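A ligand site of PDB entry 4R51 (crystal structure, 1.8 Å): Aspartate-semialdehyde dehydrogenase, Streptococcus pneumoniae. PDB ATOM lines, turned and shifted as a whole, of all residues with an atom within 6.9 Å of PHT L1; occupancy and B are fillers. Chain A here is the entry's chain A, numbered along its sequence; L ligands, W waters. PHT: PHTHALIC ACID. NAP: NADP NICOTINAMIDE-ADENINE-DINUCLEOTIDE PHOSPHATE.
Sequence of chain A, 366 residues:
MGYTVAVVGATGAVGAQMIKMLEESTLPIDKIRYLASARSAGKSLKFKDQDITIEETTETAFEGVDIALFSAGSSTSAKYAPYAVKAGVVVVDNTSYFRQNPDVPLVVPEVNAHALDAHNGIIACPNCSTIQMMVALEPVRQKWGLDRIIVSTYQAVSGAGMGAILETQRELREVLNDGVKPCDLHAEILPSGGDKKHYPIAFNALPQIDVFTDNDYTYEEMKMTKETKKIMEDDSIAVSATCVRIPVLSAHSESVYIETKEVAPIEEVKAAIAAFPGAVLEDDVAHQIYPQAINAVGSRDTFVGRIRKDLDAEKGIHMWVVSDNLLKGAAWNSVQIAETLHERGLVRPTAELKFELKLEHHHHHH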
ATOM      1  N   GLY A  73      14.240  24.037 -13.358  1.00  0.00           N
ATOM      2  CA  GLY A  73      15.345  24.992 -13.341  1.00  0.00           C
ATOM      3  C   GLY A  73      15.705  25.414 -11.932  1.00  0.00           C
ATOM      4  O   GLY A  73      14.840  25.439 -11.051  1.00  0.00           O
ATOM      5  N   SER A  74      16.977  25.733 -11.708  1.00  0.00           N
ATOM      6  CA  SER A  74      17.459  26.034 -10.377  1.00  0.00           C
ATOM      7  C   SER A  74      16.733  27.218  -9.761  1.00  0.00           C
ATOM      8  O   SER A  74      16.437  27.213  -8.565  1.00  0.00           O
ATOM      9  CB  SER A  74      18.976  26.294 -10.390  1.00  0.00           C
ATOM     10  OG  SER A  74      19.674  25.100 -10.725  1.00  0.00           O
ATOM     11  N   ASN A  94      15.654  18.018  -8.683  1.00  0.00           N
ATOM     12  CA  ASN A  94      16.621  17.621  -9.740  1.00  0.00           C
ATOM     13  C   ASN A  94      17.696  18.670 -10.074  1.00  0.00           C
ATOM     14  O   ASN A  94      18.676  18.371 -10.756  1.00  0.00           O
ATOM     15  CB  ASN A  94      15.895  17.227 -11.049  1.00  0.00           C
ATOM     16  CG  ASN A  94      15.654  15.736 -11.170  1.00  0.00           C
ATOM     17  OD1 ASN A  94      14.503  15.299 -11.285  1.00  0.00           O
ATOM     18  ND2 ASN A  94      16.732  14.947 -11.146  1.00  0.00           N
ATOM     19  N   THR A  95      17.548  19.884  -9.543  1.00  0.00           N
ATOM     20  CA  THR A  95      18.427  20.981  -9.922  1.00  0.00           C
ATOM     21  C   THR A  95      19.655  21.043  -9.006  1.00  0.00           C
ATOM     22  O   THR A  95      19.725  20.348  -7.994  1.00  0.00           O
ATOM     23  CB  THR A  95      17.706  22.354  -9.865  1.00  0.00           C
ATOM     24  OG1 THR A  95      17.709  22.839  -8.518  1.00  0.00           O
ATOM     25  CG2 THR A  95      16.273  22.237 -10.387  1.00  0.00           C
ATOM     26  N   SER A  96      20.597  21.911  -9.371  1.00  0.00           N
ATOM     27  CA  SER A  96      21.822  22.102  -8.614  1.00  0.00           C
ATOM     28  C   SER A  96      21.650  22.959  -7.356  1.00  0.00           C
ATOM     29  O   SER A  96      22.548  22.994  -6.514  1.00  0.00           O
ATOM     30  CB  SER A  96      22.901  22.735  -9.488  1.00  0.00           C
ATOM     31  OG  SER A  96      22.503  24.038  -9.911  1.00  0.00           O
ATOM     32  N   TYR A  97      20.511  23.638  -7.226  1.00  0.00           N
ATOM     33  CA  TYR A  97      20.407  24.716  -6.240  1.00  0.00           C
ATOM     34  C   TYR A  97      20.726  24.310  -4.802  1.00  0.00           C
ATOM     35  O   TYR A  97      21.499  24.998  -4.145  1.00  0.00           O
ATOM     36  CB  TYR A  97      19.046  25.414  -6.274  1.00  0.00           C
ATOM     37  CG  TYR A  97      19.104  26.728  -5.526  1.00  0.00           C
ATOM     38  CD1 TYR A  97      19.676  27.853  -6.120  1.00  0.00           C
ATOM     39  CD2 TYR A  97      18.646  26.816  -4.216  1.00  0.00           C
ATOM     40  CE1 TYR A  97      19.766  29.052  -5.423  1.00  0.00           C
ATOM     41  CE2 TYR A  97      18.744  28.009  -3.519  1.00  0.00           C
ATOM     42  CZ  TYR A  97      19.303  29.118  -4.123  1.00  0.00           C
ATOM     43  OH  TYR A  97      19.385  30.309  -3.441  1.00  0.00           O
ATOM     44  N   ARG A  99      22.034  21.308  -3.718  1.00  0.00           N
ATOM     45  CA  ARG A  99      22.866  20.094  -3.618  1.00  0.00           C
ATOM     46  C   ARG A  99      23.982  20.183  -2.576  1.00  0.00           C
ATOM     47  O   ARG A  99      24.289  19.175  -1.926  1.00  0.00           O
ATOM     48  CB  ARG A  99      23.496  19.764  -4.962  1.00  0.00           C
ATOM     49  CG  ARG A  99      22.508  19.292  -5.999  1.00  0.00           C
ATOM     50  CD  ARG A  99      23.244  18.798  -7.226  1.00  0.00           C
ATOM     51  NE  ARG A  99      22.300  18.391  -8.259  1.00  0.00           N
ATOM     52  CZ  ARG A  99      22.426  18.653  -9.556  1.00  0.00           C
ATOM     53  NH1 ARG A  99      23.492  19.297 -10.030  1.00  0.00           N
ATOM     54  NH2 ARG A  99      21.469  18.266 -10.382  1.00  0.00           N
ATOM     55  N   CYS A 125      18.625  15.444  -6.016  1.00  0.00           N
ATOM     56  CA  CYS A 125      19.126  14.511  -7.003  1.00  0.00           C
ATOM     57  C   CYS A 125      20.420  15.124  -7.570  1.00  0.00           C
ATOM     58  O   CYS A 125      20.434  16.320  -7.895  1.00  0.00           O
ATOM     59  CB  CYS A 125      18.065  14.287  -8.095  1.00  0.00           C
ATOM     60  SG  CYS A 125      18.501  13.168  -9.458  1.00  0.00           S
ATOM     61  N   PRO A 126      21.512  14.333  -7.651  1.00  0.00           N
ATOM     62  CA  PRO A 126      22.753  14.886  -8.208  1.00  0.00           C
ATOM     63  C   PRO A 126      22.697  15.120  -9.713  1.00  0.00           C
ATOM     64  O   PRO A 126      21.732  14.758 -10.387  1.00  0.00           O
ATOM     65  CB  PRO A 126      23.820  13.836  -7.867  1.00  0.00           C
ATOM     66  CG  PRO A 126      23.180  12.884  -6.914  1.00  0.00           C
ATOM     67  CD  PRO A 126      21.704  12.967  -7.142  1.00  0.00           C
ATOM     68  N   ASN A 127      23.741  15.754 -10.233  1.00  0.00           N
ATOM     69  CA  ASN A 127      23.869  15.955 -11.672  1.00  0.00           C
ATOM     70  C   ASN A 127      23.984  14.594 -12.377  1.00  0.00           C
ATOM     71  O   ASN A 127      24.603  13.678 -11.857  1.00  0.00           O
ATOM     72  CB  ASN A 127      25.083  16.815 -11.966  1.00  0.00           C
ATOM     73  CG  ASN A 127      25.284  17.037 -13.452  1.00  0.00           C
ATOM     74  OD1 ASN A 127      24.583  17.828 -14.085  1.00  0.00           O
ATOM     75  ND2 ASN A 127      26.234  16.331 -14.012  1.00  0.00           N
ATOM     76  N   CYS A 128      23.402  14.500 -13.577  1.00  0.00           N
ATOM     77  CA  CYS A 128      23.359  13.232 -14.334  1.00  0.00           C
ATOM     78  C   CYS A 128      24.732  12.590 -14.499  1.00  0.00           C
ATOM     79  O   CYS A 128      24.900  11.385 -14.270  1.00  0.00           O
ATOM     80  CB  CYS A 128      22.727  13.453 -15.701  1.00  0.00           C
ATOM     81  SG  CYS A 128      23.411  14.864 -16.563  1.00  0.00           S
ATOM     82  N   GLY A 159      20.397  16.510 -22.155  1.00  0.00           N
ATOM     83  CA  GLY A 159      20.706  17.096 -20.865  1.00  0.00           C
ATOM     84  C   GLY A 159      20.538  18.608 -20.807  1.00  0.00           C
ATOM     85  O   GLY A 159      20.409  19.165 -19.724  1.00  0.00           O
ATOM     86  N   ALA A 160      20.545  19.265 -21.972  1.00  0.00           N
ATOM     87  CA  ALA A 160      20.383  20.706 -22.063  1.00  0.00           C
ATOM     88  C   ALA A 160      18.946  21.145 -22.388  1.00  0.00           C
ATOM     89  O   ALA A 160      18.703  22.342 -22.577  1.00  0.00           O
ATOM     90  CB  ALA A 160      21.352  21.274 -23.084  1.00  0.00           C
ATOM     91  N   GLY A 161      18.018  20.207 -22.464  1.00  0.00           N
ATOM     92  CA  GLY A 161      16.596  20.518 -22.586  1.00  0.00           C
ATOM     93  C   GLY A 161      16.019  20.320 -23.967  1.00  0.00           C
ATOM     94  O   GLY A 161      16.726  20.053 -24.946  1.00  0.00           O
ATOM     95  N   ILE A 209      30.228  22.750 -20.799  1.00  0.00           N
ATOM     96  CA  ILE A 209      28.892  22.478 -20.318  1.00  0.00           C
ATOM     97  C   ILE A 209      28.679  23.379 -19.103  1.00  0.00           C
ATOM     98  O   ILE A 209      29.522  23.414 -18.210  1.00  0.00           O
ATOM     99  CB  ILE A 209      28.714  20.994 -19.974  1.00  0.00           C
ATOM    100  CG1 ILE A 209      28.742  20.169 -21.280  1.00  0.00           C
ATOM    101  CG2 ILE A 209      27.429  20.756 -19.213  1.00  0.00           C
ATOM    102  CD1 ILE A 209      28.825  18.686 -21.101  1.00  0.00           C
ATOM    103  N   ASP A 210      27.561  24.094 -19.103  1.00  0.00           N
ATOM    104  CA  ASP A 210      27.300  25.191 -18.139  1.00  0.00           C
ATOM    105  C   ASP A 210      28.312  26.322 -18.364  1.00  0.00           C
ATOM    106  O   ASP A 210      29.110  26.279 -19.290  1.00  0.00           O
ATOM    107  CB  ASP A 210      27.346  24.674 -16.705  1.00  0.00           C
ATOM    108  CG  ASP A 210      26.363  25.396 -15.776  1.00  0.00           C
ATOM    109  OD1 ASP A 210      26.251  26.637 -15.853  1.00  0.00           O
ATOM    110  OD2 ASP A 210      25.705  24.707 -14.963  1.00  0.00           O
ATOM    111  N   GLU A 220      29.730  22.572 -14.583  1.00  0.00           N
ATOM    112  CA  GLU A 220      29.453  21.145 -14.722  1.00  0.00           C
ATOM    113  C   GLU A 220      30.615  20.329 -14.149  1.00  0.00           C
ATOM    114  O   GLU A 220      30.399  19.366 -13.408  1.00  0.00           O
ATOM    115  CB  GLU A 220      29.226  20.767 -16.183  1.00  0.00           C
ATOM    116  CG  GLU A 220      28.902  19.301 -16.403  1.00  0.00           C
ATOM    117  CD  GLU A 220      27.462  18.940 -16.071  1.00  0.00           C
ATOM    118  OE1 GLU A 220      26.679  19.830 -15.646  1.00  0.00           O
ATOM    119  OE2 GLU A 220      27.119  17.740 -16.245  1.00  0.00           O
ATOM    120  N   LYS A 223      30.669  20.655 -10.375  1.00  0.00           N
ATOM    121  CA  LYS A 223      29.599  19.843  -9.803  1.00  0.00           C
ATOM    122  C   LYS A 223      30.040  18.387  -9.626  1.00  0.00           C
ATOM    123  O   LYS A 223      29.801  17.797  -8.587  1.00  0.00           O
ATOM    124  CB  LYS A 223      28.321  19.908 -10.655  1.00  0.00           C
ATOM    125  CG  LYS A 223      27.535  21.193 -10.529  1.00  0.00           C
ATOM    126  CD  LYS A 223      26.315  21.171 -11.447  1.00  0.00           C
ATOM    127  CE  LYS A 223      25.975  22.535 -12.008  1.00  0.00           C
ATOM    128  NZ  LYS A 223      24.889  22.421 -13.014  1.00  0.00           N
ATOM    129  N   GLU A 227      30.006  17.187  -5.853  1.00  0.00           N
ATOM    130  CA  GLU A 227      28.959  16.199  -5.618  1.00  0.00           C
ATOM    131  C   GLU A 227      29.542  14.830  -5.259  1.00  0.00           C
ATOM    132  O   GLU A 227      29.018  14.142  -4.375  1.00  0.00           O
ATOM    133  CB  GLU A 227      28.004  16.121  -6.820  1.00  0.00           C
ATOM    134  CG  GLU A 227      27.201  17.410  -6.988  1.00  0.00           C
ATOM    135  CD  GLU A 227      26.355  17.425  -8.234  1.00  0.00           C
ATOM    136  OE1 GLU A 227      26.104  16.334  -8.803  1.00  0.00           O
ATOM    137  OE2 GLU A 227      25.951  18.525  -8.664  1.00  0.00           O
ATOM    138  N   ARG A 245      30.232  18.247 -24.572  1.00  0.00           N
ATOM    139  CA  ARG A 245      29.009  17.926 -25.306  1.00  0.00           C
ATOM    140  C   ARG A 245      29.350  17.360 -26.675  1.00  0.00           C
ATOM    141  O   ARG A 245      30.202  17.925 -27.386  1.00  0.00           O
ATOM    142  CB  ARG A 245      28.162  19.181 -25.496  1.00  0.00           C
ATOM    143  CG  ARG A 245      26.714  18.899 -25.892  1.00  0.00           C
ATOM    144  CD  ARG A 245      25.866  18.470 -24.710  1.00  0.00           C
ATOM    145  NE  ARG A 245      25.666  19.561 -23.747  1.00  0.00           N
ATOM    146  CZ  ARG A 245      25.012  19.424 -22.601  1.00  0.00           C
ATOM    147  NH1 ARG A 245      24.471  18.253 -22.258  1.00  0.00           N
ATOM    148  NH2 ARG A 245      24.890  20.464 -21.784  1.00  0.00           N
ATOM    149  N   GLY A 329      20.158   9.342 -14.796  1.00  0.00           N
ATOM    150  CA  GLY A 329      20.729  10.663 -14.664  1.00  0.00           C
ATOM    151  C   GLY A 329      19.802  11.740 -14.151  1.00  0.00           C
ATOM    152  O   GLY A 329      20.253  12.840 -13.810  1.00  0.00           O
HETATM  153  O8  PHT L   1      23.080  20.569 -12.465  1.00  0.00           O
HETATM  154  O9  PHT L   1      21.643  19.034 -13.003  1.00  0.00           O
HETATM  155  C10 PHT L   1      21.254  23.021 -12.872  1.00  0.00           C
HETATM  156  O11 PHT L   1      22.126  23.856 -12.548  1.00  0.00           O
HETATM  157  O12 PHT L   1      20.341  22.690 -12.102  1.00  0.00           O
HETATM  158  C7  PHT L   1      22.175  20.138 -13.204  1.00  0.00           C
HETATM  159  C1  PHT L   1      20.853  23.070 -15.354  1.00  0.00           C
HETATM  160  C2  PHT L   1      21.279  22.371 -14.226  1.00  0.00           C
HETATM  161  C3  PHT L   1      21.711  20.958 -14.381  1.00  0.00           C
HETATM  162  C4  PHT L   1      21.687  20.391 -15.646  1.00  0.00           C
HETATM  163  C5  PHT L   1      21.269  21.144 -16.747  1.00  0.00           C
HETATM  164  C6  PHT L   1      20.859  22.463 -16.598  1.00  0.00           C
HETATM  165  PA  NAP L   2      13.380  21.897 -20.681  1.00  0.00           P
HETATM  166  O1A NAP L   2      13.806  23.235 -21.213  1.00  0.00           O
HETATM  167  O2A NAP L   2      13.195  20.721 -21.608  1.00  0.00           O
HETATM  168  O5B NAP L   2      12.075  22.138 -19.782  1.00  0.00           O
HETATM  169  C5B NAP L   2      11.983  23.256 -18.912  1.00  0.00           C
HETATM  170  C4B NAP L   2      10.836  23.028 -17.949  1.00  0.00           C
HETATM  171  O4B NAP L   2      10.873  24.055 -16.953  1.00  0.00           O
HETATM  172  C3B NAP L   2       9.466  23.130 -18.614  1.00  0.00           C
HETATM  173  O3B NAP L   2       8.528  22.256 -17.985  1.00  0.00           O
HETATM  174  C2B NAP L   2       9.089  24.561 -18.358  1.00  0.00           C
HETATM  175  O2B NAP L   2       7.687  24.835 -18.432  1.00  0.00           O
HETATM  176  C1B NAP L   2       9.616  24.719 -16.944  1.00  0.00           C
HETATM  177  N9A NAP L   2       9.675  26.146 -16.585  1.00  0.00           N
HETATM  178  C8A NAP L   2      10.299  27.133 -17.251  1.00  0.00           C
HETATM  179  N7A NAP L   2      10.083  28.316 -16.645  1.00  0.00           N
HETATM  180  C5A NAP L   2       9.303  28.097 -15.578  1.00  0.00           C
HETATM  181  C6A NAP L   2       8.687  28.904 -14.500  1.00  0.00           C
HETATM  182  N6A NAP L   2       8.883  30.238 -14.443  1.00  0.00           N
HETATM  183  N1A NAP L   2       7.924  28.279 -13.585  1.00  0.00           N
HETATM  184  C2A NAP L   2       7.719  26.950 -13.629  1.00  0.00           C
HETATM  185  N3A NAP L   2       8.249  26.155 -14.571  1.00  0.00           N
HETATM  186  C4A NAP L   2       9.024  26.657 -15.547  1.00  0.00           C
HETATM  187  O3  NAP L   2      14.520  21.534 -19.580  1.00  0.00           O
HETATM  188  PN  NAP L   2      14.838  20.101 -18.906  1.00  0.00           P
HETATM  189  O1N NAP L   2      15.904  19.371 -19.685  1.00  0.00           O
HETATM  190  O2N NAP L   2      13.564  19.370 -18.606  1.00  0.00           O
HETATM  191  O5D NAP L   2      15.528  20.546 -17.546  1.00  0.00           O
HETATM  192  C5D NAP L   2      14.885  21.439 -16.642  1.00  0.00           C
HETATM  193  C4D NAP L   2      15.735  21.504 -15.381  1.00  0.00           C
HETATM  194  O4D NAP L   2      15.888  20.202 -14.776  1.00  0.00           O
HETATM  195  C3D NAP L   2      17.143  21.996 -15.647  1.00  0.00           C
HETATM  196  O3D NAP L   2      17.225  23.425 -15.714  1.00  0.00           O
HETATM  197  C2D NAP L   2      17.896  21.410 -14.480  1.00  0.00           C
HETATM  198  O2D NAP L   2      17.785  22.274 -13.344  1.00  0.00           O
HETATM  199  C1D NAP L   2      17.199  20.077 -14.220  1.00  0.00           C
HETATM  200  N1N NAP L   2      17.958  18.990 -14.844  1.00  0.00           N
HETATM  201  C2N NAP L   2      18.761  18.225 -14.076  1.00  0.00           C
HETATM  202  C3N NAP L   2      19.506  17.184 -14.633  1.00  0.00           C
HETATM  203  C7N NAP L   2      20.410  16.354 -13.788  1.00  0.00           C
HETATM  204  O7N NAP L   2      21.553  16.199 -14.181  1.00  0.00           O
HETATM  205  N7N NAP L   2      19.983  15.826 -12.642  1.00  0.00           N
HETATM  206  C4N NAP L   2      19.430  16.932 -16.002  1.00  0.00           C
HETATM  207  C5N NAP L   2      18.602  17.729 -16.777  1.00  0.00           C
HETATM  208  C6N NAP L   2      17.879  18.751 -16.169  1.00  0.00           C
HETATM  209  P2B NAP L   2       6.993  25.545 -19.723  1.00  0.00           P
HETATM  210  O1X NAP L   2       6.863  24.430 -20.724  1.00  0.00           O
HETATM  211  O2X NAP L   2       5.697  26.057 -19.183  1.00  0.00           O
HETATM  212  O3X NAP L   2       7.982  26.631 -20.098  1.00  0.00           O
HETATM  213  O   HOH W   1      23.125  22.327 -19.348  1.00  0.00           O
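NZ of Lys 223 is in salt-bridge range of O8 of PHT L1 (2.6 Å).
O12 of PHT L1 lies within hydrogen-bond range of N of Ser 96.
The side-chain hydroxyl of Ser 96 lies within hydrogen-bond range of an oxygen (O11) of PHT L1.
The guanidinium group (NH2) of Arg 99 is in salt-bridge range of an oxygen (O9) of PHT L1, at 2.7 Å.
An oxygen (O12) of PHT L1 sits at hydrogen-bond distance from the side-chain hydroxyl (OG) of Ser 74 (2.9 Å).
The side-chain amide oxygen (OD1) of Asn 127 lies close to an oxygen (O9) of PHT L1, at 3.4 Å.
O7N of NAP L2 sits close to OD1 of Asn 127 (3.4 Å).
The backbone carbonyl oxygen (O) of Asn 94 lies close to a nitrogen (N7N) of NAP L2 (3.4 Å).
An oxygen (O7N) of NAP L2 is in hydrogen-bond range of the backbone NH (N) of Cys 128 (2.6 Å).
SG of Cys 128 sits at hydrogen-bond distance from O7N of NAP L2, at 3.3 Å.
The backbone carbonyl oxygen (O) of Pro 126 lies within hydrogen-bond range of a nitrogen (N7N) of NAP L2 (3.0 Å).
N7N of NAP L2 is in hydrogen-bond range of O of Gly 329, at 3.2 Å.
O12 of PHT L1 sits at hydrogen-bond distance from O2D of NAP L2 (2.9 Å).
The side-chain amino group (NZ) of Lys 223 lies within salt-bridge range of the side-chain carboxylate (OD2) of Asp 210, at 3.1 Å.
The backbone carbonyl oxygen (O) of Thr 95 is in hydrogen-bond range of the guanidinium group (NE) of Arg 99.
O of Asn 94 is in hydrogen-bond range of NH2 of Arg 99 (2.8 Å).
O of Cys 125 lies within hydrogen-bond range of NE of Arg 99 (2.8 Å).
The side-chain amide nitrogen (ND2) of Asn 127 lies within hydrogen-bond range of the side-chain carboxylate (OE2) of Glu 220 (2.8 Å).
OE1 of Glu 227 lies within hydrogen-bond range of N of Asn 127 (2.8 Å).
OG1 of Thr 95 lies within hydrogen-bond range of N of Tyr 97, 3.2 Å away.
SG of Cys 125 is in hydrogen-bond range of ND2 of Asn 94 (3.0 Å).
O of Asn 94 touches O9 of PHT L1, at 3.8 Å.
Thr 95 touches PHT L1 (CA to O12, 3.4 Å).
O of Gly 159 touches C5 of PHT L1, 3.7 Å away.
The nearest printed residue that does not touch PHT L1 is Asp 210 (4.4 Å).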
